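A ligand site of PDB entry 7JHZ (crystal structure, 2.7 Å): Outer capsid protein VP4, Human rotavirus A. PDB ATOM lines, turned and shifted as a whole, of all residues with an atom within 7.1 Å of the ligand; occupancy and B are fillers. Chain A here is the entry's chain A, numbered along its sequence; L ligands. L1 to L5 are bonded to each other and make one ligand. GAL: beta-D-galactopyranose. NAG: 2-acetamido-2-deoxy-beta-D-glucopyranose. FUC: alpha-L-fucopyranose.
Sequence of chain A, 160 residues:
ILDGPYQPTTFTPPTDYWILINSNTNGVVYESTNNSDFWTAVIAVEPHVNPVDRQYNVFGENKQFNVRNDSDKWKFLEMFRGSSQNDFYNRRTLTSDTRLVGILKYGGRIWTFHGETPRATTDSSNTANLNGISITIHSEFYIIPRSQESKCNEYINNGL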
ATOM      1  N   LYS A  75     -23.480  29.082  31.761  1.00  0.00           N
ATOM      2  CA  LYS A  75     -22.754  28.459  30.626  1.00  0.00           C
ATOM      3  C   LYS A  75     -22.663  26.950  30.889  1.00  0.00           C
ATOM      4  O   LYS A  75     -22.177  26.568  31.939  1.00  0.00           O
ATOM      5  CB  LYS A  75     -21.403  29.132  30.390  1.00  0.00           C
ATOM      6  CG  LYS A  75     -21.442  30.451  29.641  1.00  0.00           C
ATOM      7  CD  LYS A  75     -20.104  30.782  28.972  1.00  0.00           C
ATOM      8  CE  LYS A  75     -19.877  32.252  28.692  1.00  0.00           C
ATOM      9  NZ  LYS A  75     -21.085  32.922  28.150  1.00  0.00           N
ATOM     10  N   LEU A  77     -20.927  23.925  29.443  1.00  0.00           N
ATOM     11  CA  LEU A  77     -19.822  23.507  28.539  1.00  0.00           C
ATOM     12  C   LEU A  77     -19.949  22.007  28.268  1.00  0.00           C
ATOM     13  O   LEU A  77     -19.890  21.190  29.207  1.00  0.00           O
ATOM     14  CB  LEU A  77     -18.483  23.892  29.177  1.00  0.00           C
ATOM     15  CG  LEU A  77     -18.297  25.398  29.366  1.00  0.00           C
ATOM     16  CD1 LEU A  77     -17.021  25.740  30.102  1.00  0.00           C
ATOM     17  CD2 LEU A  77     -18.328  26.107  28.026  1.00  0.00           C
ATOM     18  N   ASN A  90     -13.770  21.296  24.811  1.00  0.00           N
ATOM     19  CA  ASN A  90     -15.056  22.018  24.829  1.00  0.00           C
ATOM     20  C   ASN A  90     -15.602  22.011  23.417  1.00  0.00           C
ATOM     21  O   ASN A  90     -15.195  22.868  22.636  1.00  0.00           O
ATOM     22  CB  ASN A  90     -14.862  23.432  25.363  1.00  0.00           C
ATOM     23  CG  ASN A  90     -16.161  24.198  25.430  1.00  0.00           C
ATOM     24  OD1 ASN A  90     -16.156  25.432  25.424  1.00  0.00           O
ATOM     25  ND2 ASN A  90     -17.269  23.488  25.507  1.00  0.00           N
ATOM     26  N   ARG A  91     -16.439  21.027  23.086  1.00  0.00           N
ATOM     27  CA  ARG A  91     -16.976  20.816  21.728  1.00  0.00           C
ATOM     28  C   ARG A  91     -18.085  21.843  21.457  1.00  0.00           C
ATOM     29  O   ARG A  91     -18.205  22.333  20.323  1.00  0.00           O
ATOM     30  CB  ARG A  91     -17.478  19.375  21.653  1.00  0.00           C
ATOM     31  CG  ARG A  91     -18.027  18.999  20.297  1.00  0.00           C
ATOM     32  CD  ARG A  91     -18.065  17.503  20.128  1.00  0.00           C
ATOM     33  NE  ARG A  91     -18.696  17.190  18.859  1.00  0.00           N
ATOM     34  CZ  ARG A  91     -18.908  15.959  18.404  1.00  0.00           C
ATOM     35  NH1 ARG A  91     -18.532  14.916  19.137  1.00  0.00           N
ATOM     36  NH2 ARG A  91     -19.486  15.776  17.239  1.00  0.00           N
ATOM     37  N   ARG A  92     -18.936  22.086  22.453  1.00  0.00           N
ATOM     38  CA  ARG A  92     -20.115  22.976  22.299  1.00  0.00           C
ATOM     39  C   ARG A  92     -20.330  23.758  23.584  1.00  0.00           C
ATOM     40  O   ARG A  92     -19.953  23.229  24.663  1.00  0.00           O
ATOM     41  CB  ARG A  92     -21.365  22.151  21.991  1.00  0.00           C
ATOM     42  CG  ARG A  92     -21.446  21.624  20.567  1.00  0.00           C
ATOM     43  CD  ARG A  92     -22.777  20.932  20.292  1.00  0.00           C
ATOM     44  NE  ARG A  92     -22.625  19.929  19.247  1.00  0.00           N
ATOM     45  CZ  ARG A  92     -22.129  18.708  19.435  1.00  0.00           C
ATOM     46  NH1 ARG A  92     -21.730  18.304  20.632  1.00  0.00           N
ATOM     47  NH2 ARG A  92     -22.021  17.892  18.410  1.00  0.00           N
ATOM     48  N   THR A  93     -20.974  24.908  23.497  1.00  0.00           N
ATOM     49  CA  THR A  93     -21.445  25.660  24.681  1.00  0.00           C
ATOM     50  C   THR A  93     -22.910  26.050  24.523  1.00  0.00           C
ATOM     51  O   THR A  93     -23.278  26.585  23.465  1.00  0.00           O
ATOM     52  CB  THR A  93     -20.583  26.906  24.905  1.00  0.00           C
ATOM     53  OG1 THR A  93     -19.241  26.481  25.166  1.00  0.00           O
ATOM     54  CG2 THR A  93     -21.048  27.775  26.062  1.00  0.00           C
ATOM     55  N   LEU A  94     -23.713  25.851  25.566  1.00  0.00           N
ATOM     56  CA  LEU A  94     -25.071  26.377  25.702  1.00  0.00           C
ATOM     57  C   LEU A  94     -25.068  27.514  26.728  1.00  0.00           C
ATOM     58  O   LEU A  94     -24.767  27.258  27.880  1.00  0.00           O
ATOM     59  CB  LEU A  94     -26.010  25.231  26.125  1.00  0.00           C
ATOM     60  CG  LEU A  94     -27.431  25.652  26.479  1.00  0.00           C
ATOM     61  CD1 LEU A  94     -28.085  26.371  25.292  1.00  0.00           C
ATOM     62  CD2 LEU A  94     -28.246  24.450  26.918  1.00  0.00           C
ATOM     63  N   THR A  95     -25.433  28.719  26.305  1.00  0.00           N
ATOM     64  CA  THR A  95     -25.542  29.907  27.180  1.00  0.00           C
ATOM     65  C   THR A  95     -27.025  30.163  27.430  1.00  0.00           C
ATOM     66  O   THR A  95     -27.740  30.406  26.456  1.00  0.00           O
ATOM     67  CB  THR A  95     -24.827  31.130  26.596  1.00  0.00           C
ATOM     68  OG1 THR A  95     -23.458  30.806  26.371  1.00  0.00           O
ATOM     69  CG2 THR A  95     -24.894  32.331  27.508  1.00  0.00           C
ATOM     70  N   PHE A 113     -28.624  20.796  22.631  1.00  0.00           N
ATOM     71  CA  PHE A 113     -28.817  22.222  22.269  1.00  0.00           C
ATOM     72  C   PHE A 113     -27.528  22.979  22.572  1.00  0.00           C
ATOM     73  O   PHE A 113     -26.923  22.680  23.590  1.00  0.00           O
ATOM     74  CB  PHE A 113     -30.025  22.814  22.999  1.00  0.00           C
ATOM     75  CG  PHE A 113     -31.342  22.450  22.369  1.00  0.00           C
ATOM     76  CD1 PHE A 113     -32.002  21.290  22.720  1.00  0.00           C
ATOM     77  CD2 PHE A 113     -31.917  23.273  21.408  1.00  0.00           C
ATOM     78  CE1 PHE A 113     -33.217  20.972  22.143  1.00  0.00           C
ATOM     79  CE2 PHE A 113     -33.131  22.949  20.819  1.00  0.00           C
ATOM     80  CZ  PHE A 113     -33.774  21.796  21.185  1.00  0.00           C
ATOM     81  N   HIS A 114     -27.116  23.850  21.653  1.00  0.00           N
ATOM     82  CA  HIS A 114     -26.001  24.795  21.868  1.00  0.00           C
ATOM     83  C   HIS A 114     -26.372  26.193  21.367  1.00  0.00           C
ATOM     84  O   HIS A 114     -27.434  26.379  20.776  1.00  0.00           O
ATOM     85  CB  HIS A 114     -24.692  24.253  21.283  1.00  0.00           C
ATOM     86  CG  HIS A 114     -24.570  24.310  19.808  1.00  0.00           C
ATOM     87  ND1 HIS A 114     -25.629  24.074  18.955  1.00  0.00           N
ATOM     88  CD2 HIS A 114     -23.483  24.463  19.019  1.00  0.00           C
ATOM     89  CE1 HIS A 114     -25.207  24.138  17.705  1.00  0.00           C
ATOM     90  NE2 HIS A 114     -23.906  24.368  17.723  1.00  0.00           N
ATOM     91  N   GLY A 115     -25.493  27.145  21.623  1.00  0.00           N
ATOM     92  CA  GLY A 115     -25.704  28.569  21.338  1.00  0.00           C
ATOM     93  C   GLY A 115     -26.361  29.251  22.501  1.00  0.00           C
ATOM     94  O   GLY A 115     -26.194  28.781  23.625  1.00  0.00           O
ATOM     95  N   GLU A 116     -27.054  30.355  22.274  1.00  0.00           N
ATOM     96  CA  GLU A 116     -27.499  31.261  23.361  1.00  0.00           C
ATOM     97  C   GLU A 116     -29.010  31.392  23.345  1.00  0.00           C
ATOM     98  O   GLU A 116     -29.517  31.798  22.321  1.00  0.00           O
ATOM     99  CB  GLU A 116     -26.893  32.648  23.199  1.00  0.00           C
ATOM    100  CG  GLU A 116     -27.589  33.655  24.081  1.00  0.00           C
ATOM    101  CD  GLU A 116     -26.797  34.879  24.478  1.00  0.00           C
ATOM    102  OE1 GLU A 116     -25.633  34.986  24.062  1.00  0.00           O
ATOM    103  OE2 GLU A 116     -27.355  35.725  25.214  1.00  0.00           O
ATOM    104  N   THR A 117     -29.686  31.046  24.444  1.00  0.00           N
ATOM    105  CA  THR A 117     -31.152  31.194  24.573  1.00  0.00           C
ATOM    106  C   THR A 117     -31.464  32.668  24.356  1.00  0.00           C
ATOM    107  O   THR A 117     -30.793  33.503  24.983  1.00  0.00           O
ATOM    108  CB  THR A 117     -31.648  30.638  25.918  1.00  0.00           C
ATOM    109  OG1 THR A 117     -31.180  31.496  26.957  1.00  0.00           O
ATOM    110  CG2 THR A 117     -31.208  29.220  26.172  1.00  0.00           C
ATOM    111  N   ARG A 119     -32.343  31.586  21.262  1.00  0.00           N
ATOM    112  CA  ARG A 119     -32.051  31.053  19.898  1.00  0.00           C
ATOM    113  C   ARG A 119     -31.022  29.913  19.953  1.00  0.00           C
ATOM    114  O   ARG A 119     -30.267  29.757  19.009  1.00  0.00           O
ATOM    115  CB  ARG A 119     -31.518  32.237  19.078  1.00  0.00           C
ATOM    116  CG  ARG A 119     -32.306  33.517  19.299  1.00  0.00           C
ATOM    117  CD  ARG A 119     -31.815  34.678  18.454  1.00  0.00           C
ATOM    118  NE  ARG A 119     -31.736  34.348  17.038  1.00  0.00           N
ATOM    119  CZ  ARG A 119     -32.760  34.285  16.189  1.00  0.00           C
ATOM    120  NH1 ARG A 119     -34.004  34.524  16.583  1.00  0.00           N
ATOM    121  NH2 ARG A 119     -32.532  33.966  14.925  1.00  0.00           N
ATOM    122  N   ALA A 120     -31.035  29.103  20.990  1.00  0.00           N
ATOM    123  CA  ALA A 120     -30.218  27.871  21.024  1.00  0.00           C
ATOM    124  C   ALA A 120     -30.801  26.913  19.978  1.00  0.00           C
ATOM    125  O   ALA A 120     -32.019  26.838  19.884  1.00  0.00           O
ATOM    126  CB  ALA A 120     -30.195  27.244  22.396  1.00  0.00           C
ATOM    127  N   THR A 121     -29.917  26.218  19.250  1.00  0.00           N
ATOM    128  CA  THR A 121     -30.308  25.230  18.215  1.00  0.00           C
ATOM    129  C   THR A 121     -29.745  23.855  18.564  1.00  0.00           C
ATOM    130  O   THR A 121     -28.805  23.752  19.368  1.00  0.00           O
ATOM    131  CB  THR A 121     -29.862  25.723  16.830  1.00  0.00           C
ATOM    132  OG1 THR A 121     -28.501  26.147  16.956  1.00  0.00           O
ATOM    133  CG2 THR A 121     -30.726  26.856  16.322  1.00  0.00           C
ATOM    134  N   THR A 122     -30.306  22.843  17.934  1.00  0.00           N
ATOM    135  CA  THR A 122     -29.916  21.433  18.148  1.00  0.00           C
ATOM    136  C   THR A 122     -28.680  21.113  17.276  1.00  0.00           C
ATOM    137  O   THR A 122     -28.523  21.717  16.207  1.00  0.00           O
ATOM    138  CB  THR A 122     -31.112  20.504  17.986  1.00  0.00           C
ATOM    139  OG1 THR A 122     -30.659  19.238  18.446  1.00  0.00           O
ATOM    140  CG2 THR A 122     -31.629  20.408  16.571  1.00  0.00           C
ATOM    141  N   ASP A 123     -27.814  20.239  17.762  1.00  0.00           N
ATOM    142  CA  ASP A 123     -26.651  19.746  16.998  1.00  0.00           C
ATOM    143  C   ASP A 123     -26.476  18.279  17.338  1.00  0.00           C
ATOM    144  O   ASP A 123     -27.072  17.829  18.329  1.00  0.00           O
ATOM    145  CB  ASP A 123     -25.405  20.589  17.266  1.00  0.00           C
ATOM    146  CG  ASP A 123     -24.288  20.382  16.261  1.00  0.00           C
ATOM    147  OD1 ASP A 123     -24.603  20.121  15.066  1.00  0.00           O
ATOM    148  OD2 ASP A 123     -23.109  20.462  16.690  1.00  0.00           O
ATOM    149  N   SER A 124     -25.729  17.562  16.519  1.00  0.00           N
ATOM    150  CA  SER A 124     -25.625  16.087  16.589  1.00  0.00           C
ATOM    151  C   SER A 124     -24.167  15.678  16.778  1.00  0.00           C
ATOM    152  O   SER A 124     -23.301  16.356  16.284  1.00  0.00           O
ATOM    153  CB  SER A 124     -26.213  15.447  15.354  1.00  0.00           C
ATOM    154  OG  SER A 124     -25.606  15.951  14.185  1.00  0.00           O
ATOM    155  N   SER A 125     -23.956  14.589  17.498  1.00  0.00           N
ATOM    156  CA  SER A 125     -22.656  13.871  17.597  1.00  0.00           C
ATOM    157  C   SER A 125     -22.905  12.456  17.096  1.00  0.00           C
ATOM    158  O   SER A 125     -23.927  11.883  17.503  1.00  0.00           O
ATOM    159  CB  SER A 125     -22.145  13.867  19.018  1.00  0.00           C
ATOM    160  OG  SER A 125     -21.910  15.192  19.479  1.00  0.00           O
HETATM  161  C1  GAL L   1     -20.487  21.931  15.439  1.00  0.00           C
HETATM  162  C2  GAL L   1     -21.451  23.147  15.528  1.00  0.00           C
HETATM  163  C3  GAL L   1     -20.859  24.444  15.038  1.00  0.00           C
HETATM  164  C4  GAL L   1     -19.940  24.297  13.774  1.00  0.00           C
HETATM  165  C5  GAL L   1     -19.331  22.887  13.646  1.00  0.00           C
HETATM  166  C6  GAL L   1     -17.959  22.932  12.945  1.00  0.00           C
HETATM  167  O1  GAL L   1     -20.242  21.400  16.722  1.00  0.00           O
HETATM  168  O2  GAL L   1     -22.627  22.939  14.728  1.00  0.00           O
HETATM  169  O3  GAL L   1     -20.137  24.925  16.110  1.00  0.00           O
HETATM  170  O4  GAL L   1     -18.909  25.332  13.815  1.00  0.00           O
HETATM  171  O5  GAL L   1     -19.187  22.291  14.939  1.00  0.00           O
HETATM  172  O6  GAL L   1     -17.856  21.883  11.970  1.00  0.00           O
HETATM  173  C1  NAG L   2     -20.332  26.208  16.745  1.00  0.00           C
HETATM  174  C2  NAG L   2     -21.505  27.183  16.453  1.00  0.00           C
HETATM  175  C3  NAG L   2     -21.181  28.387  17.336  1.00  0.00           C
HETATM  176  C4  NAG L   2     -21.097  27.940  18.814  1.00  0.00           C
HETATM  177  C5  NAG L   2     -20.115  26.802  18.948  1.00  0.00           C
HETATM  178  C6  NAG L   2     -20.126  26.151  20.328  1.00  0.00           C
HETATM  179  C7  NAG L   2     -22.576  27.280  14.189  1.00  0.00           C
HETATM  180  C8  NAG L   2     -22.407  27.798  12.762  1.00  0.00           C
HETATM  181  N2  NAG L   2     -21.571  27.626  15.041  1.00  0.00           N
HETATM  182  O3  NAG L   2     -22.178  29.379  17.219  1.00  0.00           O
HETATM  183  O4  NAG L   2     -20.675  29.042  19.645  1.00  0.00           O
HETATM  184  O5  NAG L   2     -20.520  25.770  18.064  1.00  0.00           O
HETATM  185  O6  NAG L   2     -21.475  25.913  20.766  1.00  0.00           O
HETATM  186  O7  NAG L   2     -23.542  26.545  14.472  1.00  0.00           O
HETATM  187  C1  GAL L   3     -21.714  30.666  16.673  1.00  0.00           C
HETATM  188  C2  GAL L   3     -22.964  31.570  16.527  1.00  0.00           C
HETATM  189  C3  GAL L   3     -22.612  32.916  15.950  1.00  0.00           C
HETATM  190  C4  GAL L   3     -21.509  33.596  16.742  1.00  0.00           C
HETATM  191  C5  GAL L   3     -20.284  32.679  16.851  1.00  0.00           C
HETATM  192  C6  GAL L   3     -19.199  33.519  17.601  1.00  0.00           C
HETATM  193  O2  GAL L   3     -23.915  30.968  15.640  1.00  0.00           O
HETATM  194  O3  GAL L   3     -23.765  33.679  16.073  1.00  0.00           O
HETATM  195  O4  GAL L   3     -22.000  33.931  18.079  1.00  0.00           O
HETATM  196  O5  GAL L   3     -20.666  31.376  17.476  1.00  0.00           O
HETATM  197  O6  GAL L   3     -18.055  32.727  17.965  1.00  0.00           O
HETATM  198  C1  FUC L   4     -21.353  29.137  20.906  1.00  0.00           C
HETATM  199  C2  FUC L   4     -20.458  29.832  21.893  1.00  0.00           C
HETATM  200  C3  FUC L   4     -20.288  31.298  21.538  1.00  0.00           C
HETATM  201  C4  FUC L   4     -21.627  32.015  21.419  1.00  0.00           C
HETATM  202  C5  FUC L   4     -22.518  31.264  20.426  1.00  0.00           C
HETATM  203  C6  FUC L   4     -23.945  31.856  20.424  1.00  0.00           C
HETATM  204  O2  FUC L   4     -19.173  29.193  21.901  1.00  0.00           O
HETATM  205  O3  FUC L   4     -19.525  31.907  22.573  1.00  0.00           O
HETATM  206  O4  FUC L   4     -22.229  32.076  22.711  1.00  0.00           O
HETATM  207  O5  FUC L   4     -22.591  29.848  20.778  1.00  0.00           O
HETATM  208  C1  FUC L   5     -25.272  30.953  16.134  1.00  0.00           C
HETATM  209  C2  FUC L   5     -26.266  30.660  14.972  1.00  0.00           C
HETATM  210  C3  FUC L   5     -26.139  29.210  14.528  1.00  0.00           C
HETATM  211  C4  FUC L   5     -26.359  28.293  15.769  1.00  0.00           C
HETATM  212  C5  FUC L   5     -25.239  28.600  16.736  1.00  0.00           C
HETATM  213  C6  FUC L   5     -25.284  27.636  17.932  1.00  0.00           C
HETATM  214  O2  FUC L   5     -26.007  31.532  13.848  1.00  0.00           O
HETATM  215  O3  FUC L   5     -27.087  28.937  13.486  1.00  0.00           O
HETATM  216  O4  FUC L   5     -27.675  28.537  16.471  1.00  0.00           O
HETATM  217  O5  FUC L   5     -25.407  29.961  17.184  1.00  0.00           O
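The side-chain carboxylate of Asp 123 lies within salt-bridge range of the guanidinium group of Arg 92 (2.7 Å).
The side-chain hydroxyl (OG1) of Thr 93 sits at hydrogen-bond distance from the side-chain amide oxygen (OD1) of Asn 90, at 3.3 Å.
O of Thr 121 lies within hydrogen-bond range of N of His 114 (2.8 Å).
The backbone carbonyl oxygen of Thr 93 sits at hydrogen-bond distance from the backbone NH of Gly 115, 2.9 Å away.
O of Gly 115 sits at hydrogen-bond distance from N of Thr 95 (2.8 Å).
NH2 of Arg 92 is in hydrogen-bond range of OG of Ser 125 (2.9 Å).
The backbone carbonyl oxygen (O) of Ser 124 sits at hydrogen-bond distance from the guanidinium group (NH2) of Arg 92 (2.9 Å).
The backbone carbonyl oxygen (O) of Arg 92 sits at hydrogen-bond distance from the side-chain amide nitrogen (ND2) of Asn 90, 2.8 Å away.
Residues that only touch the ligand: His 114 (3.0 Å), Gly 115 (3.4 Å), Arg 92 (3.6 Å), Arg 119 (3.8 Å) and Glu 116 (3.9 Å).
Hydrophobic or aromatic side chains that line the ligand: His 114.
Of the 20 residues printed, 8 come within 4 Å of the ligand.
The side-chain hydroxyl of Thr 121 is in hydrogen-bond range of an oxygen (O4) of FUC L5 (2.6 Å).
O6 of NAG L2 sits at hydrogen-bond distance from O of Thr 93, at 3.3 Å.
The side-chain carboxylate (OD2) of Asp 123 is in hydrogen-bond range of an oxygen (O1) of GAL L1, 3.0 Å away.
The backbone NH (N) of Thr 93 sits at hydrogen-bond distance from an oxygen (O6) of NAG L2 (3.0 Å).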
